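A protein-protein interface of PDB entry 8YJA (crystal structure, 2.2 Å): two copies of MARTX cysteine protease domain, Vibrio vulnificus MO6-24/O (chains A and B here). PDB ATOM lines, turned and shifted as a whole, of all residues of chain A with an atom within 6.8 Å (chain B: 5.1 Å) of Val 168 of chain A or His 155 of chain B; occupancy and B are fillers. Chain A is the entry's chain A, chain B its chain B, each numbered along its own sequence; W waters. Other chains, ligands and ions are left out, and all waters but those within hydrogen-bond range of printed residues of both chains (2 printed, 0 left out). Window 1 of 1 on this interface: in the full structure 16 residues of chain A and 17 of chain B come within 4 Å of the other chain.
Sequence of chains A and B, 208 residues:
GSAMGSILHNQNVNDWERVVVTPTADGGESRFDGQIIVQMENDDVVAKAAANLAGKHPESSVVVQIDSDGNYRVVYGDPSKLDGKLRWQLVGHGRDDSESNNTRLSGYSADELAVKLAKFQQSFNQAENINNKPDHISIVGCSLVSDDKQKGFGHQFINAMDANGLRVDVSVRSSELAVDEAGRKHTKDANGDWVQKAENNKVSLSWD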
ATOM      1  N   LYS A 133      22.956 -31.822 -36.544  1.00  0.00           N
ATOM      2  CA  LYS A 133      23.039 -31.435 -35.143  1.00  0.00           C
ATOM      3  C   LYS A 133      23.040 -32.683 -34.255  1.00  0.00           C
ATOM      4  O   LYS A 133      22.255 -33.612 -34.497  1.00  0.00           O
ATOM      5  CB  LYS A 133      21.846 -30.548 -34.790  1.00  0.00           C
ATOM      6  CG  LYS A 133      20.540 -31.313 -35.028  1.00  0.00           C
ATOM      7  CD  LYS A 133      19.257 -30.621 -34.644  1.00  0.00           C
ATOM      8  CE  LYS A 133      18.112 -31.495 -35.142  1.00  0.00           C
ATOM      9  NZ  LYS A 133      18.551 -32.330 -36.325  1.00  0.00           N
ATOM     10  N   PRO A 134      23.923 -32.771 -33.266  1.00  0.00           N
ATOM     11  CA  PRO A 134      23.842 -33.885 -32.315  1.00  0.00           C
ATOM     12  C   PRO A 134      22.710 -33.662 -31.323  1.00  0.00           C
ATOM     13  O   PRO A 134      22.468 -32.540 -30.874  1.00  0.00           O
ATOM     14  CB  PRO A 134      25.207 -33.856 -31.617  1.00  0.00           C
ATOM     15  CG  PRO A 134      25.620 -32.409 -31.699  1.00  0.00           C
ATOM     16  CD  PRO A 134      25.092 -31.907 -33.016  1.00  0.00           C
ATOM     17  N   ASP A 135      22.011 -34.746 -30.981  1.00  0.00           N
ATOM     18  CA  ASP A 135      21.017 -34.673 -29.918  1.00  0.00           C
ATOM     19  C   ASP A 135      21.673 -34.683 -28.547  1.00  0.00           C
ATOM     20  O   ASP A 135      21.119 -34.140 -27.585  1.00  0.00           O
ATOM     21  CB  ASP A 135      20.024 -35.839 -30.054  1.00  0.00           C
ATOM     22  CG  ASP A 135      19.175 -36.057 -28.795  1.00  0.00           C
ATOM     23  OD1 ASP A 135      19.634 -36.763 -27.868  1.00  0.00           O
ATOM     24  OD2 ASP A 135      18.039 -35.534 -28.736  1.00  0.00           O
ATOM     25  N   HIS A 136      22.848 -35.288 -28.435  1.00  0.00           N
ATOM     26  CA  HIS A 136      23.377 -35.628 -27.126  1.00  0.00           C
ATOM     27  C   HIS A 136      24.897 -35.578 -27.165  1.00  0.00           C
ATOM     28  O   HIS A 136      25.521 -36.000 -28.141  1.00  0.00           O
ATOM     29  CB  HIS A 136      22.887 -37.016 -26.693  1.00  0.00           C
ATOM     30  CG  HIS A 136      23.268 -37.380 -25.293  1.00  0.00           C
ATOM     31  ND1 HIS A 136      22.366 -37.383 -24.252  1.00  0.00           N
ATOM     32  CD2 HIS A 136      24.459 -37.744 -24.761  1.00  0.00           C
ATOM     33  CE1 HIS A 136      22.981 -37.734 -23.138  1.00  0.00           C
ATOM     34  NE2 HIS A 136      24.252 -37.960 -23.422  1.00  0.00           N
ATOM     35  N   ILE A 137      25.480 -35.063 -26.093  1.00  0.00           N
ATOM     36  CA  ILE A 137      26.922 -34.952 -25.955  1.00  0.00           C
ATOM     37  C   ILE A 137      27.278 -35.577 -24.619  1.00  0.00           C
ATOM     38  O   ILE A 137      26.763 -35.150 -23.579  1.00  0.00           O
ATOM     39  CB  ILE A 137      27.385 -33.484 -26.018  1.00  0.00           C
ATOM     40  CG1 ILE A 137      26.970 -32.871 -27.358  1.00  0.00           C
ATOM     41  CG2 ILE A 137      28.895 -33.375 -25.785  1.00  0.00           C
ATOM     42  CD1 ILE A 137      27.761 -31.673 -27.771  1.00  0.00           C
ATOM     43  N   HIS A 155      27.333 -28.226 -16.885  1.00  0.00           N
ATOM     44  CA  HIS A 155      26.318 -27.170 -16.814  1.00  0.00           C
ATOM     45  C   HIS A 155      26.735 -25.951 -17.628  1.00  0.00           C
ATOM     46  O   HIS A 155      25.947 -25.422 -18.423  1.00  0.00           O
ATOM     47  CB  HIS A 155      26.075 -26.786 -15.352  1.00  0.00           C
ATOM     48  CG  HIS A 155      24.732 -26.163 -15.096  1.00  0.00           C
ATOM     49  ND1 HIS A 155      24.019 -25.488 -16.067  1.00  0.00           N
ATOM     50  CD2 HIS A 155      23.979 -26.107 -13.971  1.00  0.00           C
ATOM     51  CE1 HIS A 155      22.887 -25.046 -15.552  1.00  0.00           C
ATOM     52  NE2 HIS A 155      22.836 -25.408 -14.282  1.00  0.00           N
ATOM     53  N   PHE A 157      28.855 -25.947 -20.075  1.00  0.00           N
ATOM     54  CA  PHE A 157      28.903 -26.395 -21.460  1.00  0.00           C
ATOM     55  C   PHE A 157      27.526 -26.367 -22.095  1.00  0.00           C
ATOM     56  O   PHE A 157      27.378 -25.930 -23.245  1.00  0.00           O
ATOM     57  CB  PHE A 157      29.496 -27.809 -21.507  1.00  0.00           C
ATOM     58  CG  PHE A 157      29.674 -28.348 -22.890  1.00  0.00           C
ATOM     59  CD1 PHE A 157      30.680 -27.869 -23.710  1.00  0.00           C
ATOM     60  CD2 PHE A 157      28.854 -29.349 -23.363  1.00  0.00           C
ATOM     61  CE1 PHE A 157      30.861 -28.374 -24.983  1.00  0.00           C
ATOM     62  CE2 PHE A 157      29.035 -29.864 -24.638  1.00  0.00           C
ATOM     63  CZ  PHE A 157      30.037 -29.373 -25.447  1.00  0.00           C
ATOM     64  N   ILE A 158      26.503 -26.827 -21.360  1.00  0.00           N
ATOM     65  CA  ILE A 158      25.127 -26.725 -21.850  1.00  0.00           C
ATOM     66  C   ILE A 158      24.805 -25.277 -22.190  1.00  0.00           C
ATOM     67  O   ILE A 158      24.280 -24.976 -23.267  1.00  0.00           O
ATOM     68  CB  ILE A 158      24.125 -27.263 -20.808  1.00  0.00           C
ATOM     69  CG1 ILE A 158      24.040 -28.773 -20.806  1.00  0.00           C
ATOM     70  CG2 ILE A 158      22.729 -26.719 -21.078  1.00  0.00           C
ATOM     71  CD1 ILE A 158      23.970 -29.356 -19.395  1.00  0.00           C
ATOM     72  N   ASN A 159      25.116 -24.361 -21.269  1.00  0.00           N
ATOM     73  CA  ASN A 159      24.714 -22.968 -21.444  1.00  0.00           C
ATOM     74  C   ASN A 159      25.368 -22.359 -22.678  1.00  0.00           C
ATOM     75  O   ASN A 159      24.692 -21.756 -23.524  1.00  0.00           O
ATOM     76  CB  ASN A 159      25.063 -22.166 -20.194  1.00  0.00           C
ATOM     77  CG  ASN A 159      24.164 -22.512 -19.004  1.00  0.00           C
ATOM     78  OD1 ASN A 159      23.074 -23.079 -19.163  1.00  0.00           O
ATOM     79  ND2 ASN A 159      24.626 -22.172 -17.805  1.00  0.00           N
ATOM     80  N   MET A 161      26.574 -23.951 -25.275  1.00  0.00           N
ATOM     81  CA  MET A 161      26.018 -24.591 -26.464  1.00  0.00           C
ATOM     82  C   MET A 161      24.624 -24.063 -26.764  1.00  0.00           C
ATOM     83  O   MET A 161      24.299 -23.764 -27.921  1.00  0.00           O
ATOM     84  CB  MET A 161      25.966 -26.110 -26.286  1.00  0.00           C
ATOM     85  CG  MET A 161      27.310 -26.812 -26.327  1.00  0.00           C
ATOM     86  SD  MET A 161      28.206 -26.453 -27.836  1.00  0.00           S
ATOM     87  CE  MET A 161      28.296 -28.080 -28.582  1.00  0.00           C
ATOM     88  N   ASP A 162      23.785 -23.950 -25.728  1.00  0.00           N
ATOM     89  CA  ASP A 162      22.401 -23.549 -25.935  1.00  0.00           C
ATOM     90  C   ASP A 162      22.317 -22.086 -26.355  1.00  0.00           C
ATOM     91  O   ASP A 162      21.467 -21.727 -27.181  1.00  0.00           O
ATOM     92  CB  ASP A 162      21.588 -23.840 -24.663  1.00  0.00           C
ATOM     93  CG  ASP A 162      20.333 -22.971 -24.534  1.00  0.00           C
ATOM     94  OD1 ASP A 162      19.574 -22.856 -25.519  1.00  0.00           O
ATOM     95  OD2 ASP A 162      20.079 -22.430 -23.430  1.00  0.00           O
ATOM     96  N   LEU A 166      22.869 -24.396 -30.298  1.00  0.00           N
ATOM     97  CA  LEU A 166      23.115 -25.834 -30.359  1.00  0.00           C
ATOM     98  C   LEU A 166      22.595 -26.432 -29.049  1.00  0.00           C
ATOM     99  O   LEU A 166      23.330 -26.545 -28.062  1.00  0.00           O
ATOM    100  CB  LEU A 166      24.600 -26.088 -30.585  1.00  0.00           C
ATOM    101  CG  LEU A 166      25.037 -27.330 -31.378  1.00  0.00           C
ATOM    102  CD1 LEU A 166      26.406 -27.125 -32.018  1.00  0.00           C
ATOM    103  CD2 LEU A 166      25.072 -28.555 -30.494  1.00  0.00           C
ATOM    104  N   ARG A 167      21.306 -26.793 -29.039  1.00  0.00           N
ATOM    105  CA  ARG A 167      20.639 -27.277 -27.832  1.00  0.00           C
ATOM    106  C   ARG A 167      20.698 -28.801 -27.783  1.00  0.00           C
ATOM    107  O   ARG A 167      20.123 -29.487 -28.637  1.00  0.00           O
ATOM    108  CB  ARG A 167      19.191 -26.785 -27.768  1.00  0.00           C
ATOM    109  CG  ARG A 167      19.010 -25.406 -28.376  1.00  0.00           C
ATOM    110  CD  ARG A 167      18.054 -24.522 -27.577  1.00  0.00           C
ATOM    111  NE  ARG A 167      16.645 -24.885 -27.664  1.00  0.00           N
ATOM    112  CZ  ARG A 167      15.755 -24.627 -26.713  1.00  0.00           C
ATOM    113  NH1 ARG A 167      16.106 -24.049 -25.572  1.00  0.00           N
ATOM    114  NH2 ARG A 167      14.479 -24.932 -26.920  1.00  0.00           N
ATOM    115  N   VAL A 168      21.408 -29.322 -26.784  1.00  0.00           N
ATOM    116  CA  VAL A 168      21.646 -30.750 -26.648  1.00  0.00           C
ATOM    117  C   VAL A 168      21.510 -31.146 -25.188  1.00  0.00           C
ATOM    118  O   VAL A 168      21.638 -30.323 -24.277  1.00  0.00           O
ATOM    119  CB  VAL A 168      23.047 -31.163 -27.152  1.00  0.00           C
ATOM    120  CG1 VAL A 168      23.238 -30.759 -28.590  1.00  0.00           C
ATOM    121  CG2 VAL A 168      24.105 -30.557 -26.294  1.00  0.00           C
ATOM    122  N   ASP A 169      21.280 -32.438 -24.974  1.00  0.00           N
ATOM    123  CA  ASP A 169      21.446 -33.009 -23.648  1.00  0.00           C
ATOM    124  C   ASP A 169      22.924 -33.298 -23.425  1.00  0.00           C
ATOM    125  O   ASP A 169      23.632 -33.718 -24.341  1.00  0.00           O
ATOM    126  CB  ASP A 169      20.633 -34.300 -23.490  1.00  0.00           C
ATOM    127  CG  ASP A 169      19.121 -34.067 -23.593  1.00  0.00           C
ATOM    128  OD1 ASP A 169      18.406 -34.966 -24.109  1.00  0.00           O
ATOM    129  OD2 ASP A 169      18.663 -32.955 -23.244  1.00  0.00           O
ATOM    130  N   VAL A 170      23.389 -33.084 -22.207  1.00  0.00           N
ATOM    131  CA  VAL A 170      24.791 -33.273 -21.870  1.00  0.00           C
ATOM    132  C   VAL A 170      24.873 -34.157 -20.641  1.00  0.00           C
ATOM    133  O   VAL A 170      24.124 -33.965 -19.677  1.00  0.00           O
ATOM    134  CB  VAL A 170      25.489 -31.916 -21.621  1.00  0.00           C
ATOM    135  CG1 VAL A 170      26.851 -32.105 -21.049  1.00  0.00           C
ATOM    136  CG2 VAL A 170      25.558 -31.113 -22.913  1.00  0.00           C
ATOM    137  N   LYS B 151      14.153 -30.093 -25.184  1.00  0.00           N
ATOM    138  CA  LYS B 151      15.410 -29.623 -24.608  1.00  0.00           C
ATOM    139  C   LYS B 151      15.200 -28.342 -23.819  1.00  0.00           C
ATOM    140  O   LYS B 151      15.815 -28.151 -22.761  1.00  0.00           O
ATOM    141  CB  LYS B 151      16.452 -29.407 -25.705  1.00  0.00           C
ATOM    142  CG  LYS B 151      16.672 -30.613 -26.598  1.00  0.00           C
ATOM    143  CD  LYS B 151      17.578 -31.619 -25.925  1.00  0.00           C
ATOM    144  CE  LYS B 151      17.940 -32.748 -26.874  1.00  0.00           C
ATOM    145  NZ  LYS B 151      17.341 -34.035 -26.392  1.00  0.00           N
ATOM    146  N   GLY B 152      14.330 -27.457 -24.310  1.00  0.00           N
ATOM    147  CA  GLY B 152      14.009 -26.259 -23.549  1.00  0.00           C
ATOM    148  C   GLY B 152      13.534 -26.583 -22.145  1.00  0.00           C
ATOM    149  O   GLY B 152      14.036 -26.024 -21.165  1.00  0.00           O
ATOM    150  N   PHE B 153      12.595 -27.532 -22.024  1.00  0.00           N
ATOM    151  CA  PHE B 153      12.157 -27.951 -20.694  1.00  0.00           C
ATOM    152  C   PHE B 153      13.316 -28.531 -19.894  1.00  0.00           C
ATOM    153  O   PHE B 153      13.466 -28.235 -18.703  1.00  0.00           O
ATOM    154  CB  PHE B 153      11.014 -28.969 -20.792  1.00  0.00           C
ATOM    155  CG  PHE B 153      10.351 -29.265 -19.463  1.00  0.00           C
ATOM    156  CD1 PHE B 153      10.862 -30.240 -18.609  1.00  0.00           C
ATOM    157  CD2 PHE B 153       9.232 -28.547 -19.053  1.00  0.00           C
ATOM    158  CE1 PHE B 153      10.259 -30.507 -17.382  1.00  0.00           C
ATOM    159  CE2 PHE B 153       8.629 -28.802 -17.825  1.00  0.00           C
ATOM    160  CZ  PHE B 153       9.142 -29.786 -16.991  1.00  0.00           C
ATOM    161  N   GLY B 154      14.152 -29.357 -20.537  1.00  0.00           N
ATOM    162  CA  GLY B 154      15.259 -29.985 -19.825  1.00  0.00           C
ATOM    163  C   GLY B 154      16.254 -28.987 -19.264  1.00  0.00           C
ATOM    164  O   GLY B 154      16.682 -29.105 -18.114  1.00  0.00           O
ATOM    165  N   HIS B 155      16.632 -27.984 -20.056  1.00  0.00           N
ATOM    166  CA  HIS B 155      17.581 -26.987 -19.564  1.00  0.00           C
ATOM    167  C   HIS B 155      16.953 -26.104 -18.488  1.00  0.00           C
ATOM    168  O   HIS B 155      17.613 -25.770 -17.497  1.00  0.00           O
ATOM    169  CB  HIS B 155      18.121 -26.157 -20.732  1.00  0.00           C
ATOM    170  CG  HIS B 155      18.777 -26.985 -21.799  1.00  0.00           C
ATOM    171  ND1 HIS B 155      19.096 -28.318 -21.616  1.00  0.00           N
ATOM    172  CD2 HIS B 155      19.137 -26.684 -23.071  1.00  0.00           C
ATOM    173  CE1 HIS B 155      19.636 -28.793 -22.725  1.00  0.00           C
ATOM    174  NE2 HIS B 155      19.669 -27.824 -23.624  1.00  0.00           N
ATOM    175  N   GLN B 156      15.670 -25.755 -18.633  1.00  0.00           N
ATOM    176  CA  GLN B 156      14.948 -25.147 -17.516  1.00  0.00           C
ATOM    177  C   GLN B 156      15.017 -26.032 -16.280  1.00  0.00           C
ATOM    178  O   GLN B 156      15.321 -25.564 -15.174  1.00  0.00           O
ATOM    179  CB  GLN B 156      13.484 -24.906 -17.897  1.00  0.00           C
ATOM    180  CG  GLN B 156      13.231 -23.788 -18.895  1.00  0.00           C
ATOM    181  CD  GLN B 156      11.752 -23.659 -19.287  1.00  0.00           C
ATOM    182  OE1 GLN B 156      10.883 -24.334 -18.726  1.00  0.00           O
ATOM    183  NE2 GLN B 156      11.467 -22.789 -20.259  1.00  0.00           N
ATOM    184  N   PHE B 157      14.741 -27.328 -16.452  1.00  0.00           N
ATOM    185  CA  PHE B 157      14.714 -28.243 -15.313  1.00  0.00           C
ATOM    186  C   PHE B 157      16.086 -28.356 -14.644  1.00  0.00           C
ATOM    187  O   PHE B 157      16.172 -28.452 -13.415  1.00  0.00           O
ATOM    188  CB  PHE B 157      14.198 -29.614 -15.772  1.00  0.00           C
ATOM    189  CG  PHE B 157      14.208 -30.672 -14.702  1.00  0.00           C
ATOM    190  CD1 PHE B 157      13.332 -30.609 -13.630  1.00  0.00           C
ATOM    191  CD2 PHE B 157      15.080 -31.750 -14.786  1.00  0.00           C
ATOM    192  CE1 PHE B 157      13.347 -31.597 -12.646  1.00  0.00           C
ATOM    193  CE2 PHE B 157      15.099 -32.739 -13.803  1.00  0.00           C
ATOM    194  CZ  PHE B 157      14.235 -32.663 -12.740  1.00  0.00           C
ATOM    195  N   ILE B 158      17.172 -28.350 -15.426  1.00  0.00           N
ATOM    196  CA  ILE B 158      18.509 -28.431 -14.831  1.00  0.00           C
ATOM    197  C   ILE B 158      18.730 -27.268 -13.875  1.00  0.00           C
ATOM    198  O   ILE B 158      19.158 -27.454 -12.729  1.00  0.00           O
ATOM    199  CB  ILE B 158      19.599 -28.453 -15.917  1.00  0.00           C
ATOM    200  CG1 ILE B 158      19.449 -29.668 -16.812  1.00  0.00           C
ATOM    201  CG2 ILE B 158      20.971 -28.479 -15.278  1.00  0.00           C
ATOM    202  CD1 ILE B 158      20.442 -29.711 -17.956  1.00  0.00           C
ATOM    203  N   ASN B 159      18.448 -26.049 -14.341  1.00  0.00           N
ATOM    204  CA  ASN B 159      18.611 -24.876 -13.492  1.00  0.00           C
ATOM    205  C   ASN B 159      17.716 -24.968 -12.269  1.00  0.00           C
ATOM    206  O   ASN B 159      18.158 -24.723 -11.140  1.00  0.00           O
ATOM    207  CB  ASN B 159      18.302 -23.614 -14.291  1.00  0.00           C
ATOM    208  CG  ASN B 159      19.197 -23.465 -15.488  1.00  0.00           C
ATOM    209  OD1 ASN B 159      20.343 -23.896 -15.462  1.00  0.00           O
ATOM    210  ND2 ASN B 159      18.685 -22.860 -16.549  1.00  0.00           N
HETATM  211  O   HOH W   1      16.626 -37.301 -26.985  1.00  0.00           O
HETATM  212  O   HOH W   2      22.472 -27.070 -25.157  1.00  0.00           O
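The backbone NH (N) of Asp 169 of chain A sits at hydrogen-bond distance from the backbone carbonyl oxygen (O) of Asp 135 of chain A (3.1 Å). N of Ile 137 of chain A is in hydrogen-bond range of O of Asp 169 of chain A (2.9 Å). The side-chain carboxylate of Asp 162 of chain A lies within salt-bridge range of the guanidinium group of Arg 167 of chain A, at 3.7 Å. A ring nitrogen (ND1) of His 155 of chain B lies close to the backbone carbonyl oxygen (O) of Lys 151 of chain B (3.5 Å). O of His 155 of chain B sits at hydrogen-bond distance from ND2 of Asn 159 of chain B (3.2 Å).
Water W1 lies within hydrogen-bond range of OD2 of Asp 135 of chain A (2.9 Å) and NZ of Lys 151 of chain B (3.4 Å). Water W2 lies within hydrogen-bond range of N of Val 168 of chain A, O of Leu 166 of chain A, NE2 of His 155 of chain B, O of Ile 158 of chain A and N of Asp 162 of chain A.
His 155 of chain A touches Ile 158 of chain B, but with the chains exchanged Ile 158 of chain A does not touch His 155 of chain B (4.01 Å). His 155 of chain A touches Asn 159 of chain B, but with the chains exchanged Asn 159 of chain A does not touch His 155 of chain B (6.0 Å). Ile 158 of chain B touches its own counterpart, Ile 158 of chain A. 4 positions are printed for both chains. Of the 7 pairs that touch across the chains among the printed residues, 1 has its exchanged pair printed and touching as well.
Printed residues of chain B that touch a printed residue of chain A: Lys 151, Gly 152, His 155, Ile 158 and Asn 159. Among the printed residues, 7 pairs touch across the chains.
OD2 of Asp 135 of chain A is in salt-bridge range of NZ of Lys 151 of chain B (2.9 Å). NE2 of His 155 of chain A lies close to OD1 of Asn 159 of chain B (3.1 Å). NE2 of His 155 of chain B sits close to O of Val 168 of chain A, 3.2 Å away. OD1 of Asp 169 of chain A lies within salt-bridge range of NZ of Lys 151 of chain B.
Of chain B, only His 155 (3.0 Å) comes within 4 Å of Val 168 of chain A. Printed residues of chain A within 4 Å of His 155 of chain B: Val 168. Of the printed residues of chain A, Gly 152 of chain B touches Arg 167. Of the printed residues of chain B, Arg 167 of chain A touches Gly 152. Phe 157 of chain B touches none of the printed residues of chain A. Met 161 of chain A touches none of the printed residues of chain B. The nearest printed residue of chain B that does not touch Asp 169 of chain A is His 155 of chain B (4.3 Å).
NE2 of His 155 of chain A touches CG2 of Ile 158 of chain B, 3.7 Å away. CD1 of Ile 158 of chain B touches CD1 of Ile 158 of chain A, 3.8 Å away. Arg 167 of chain A touches Gly 152 of chain B.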
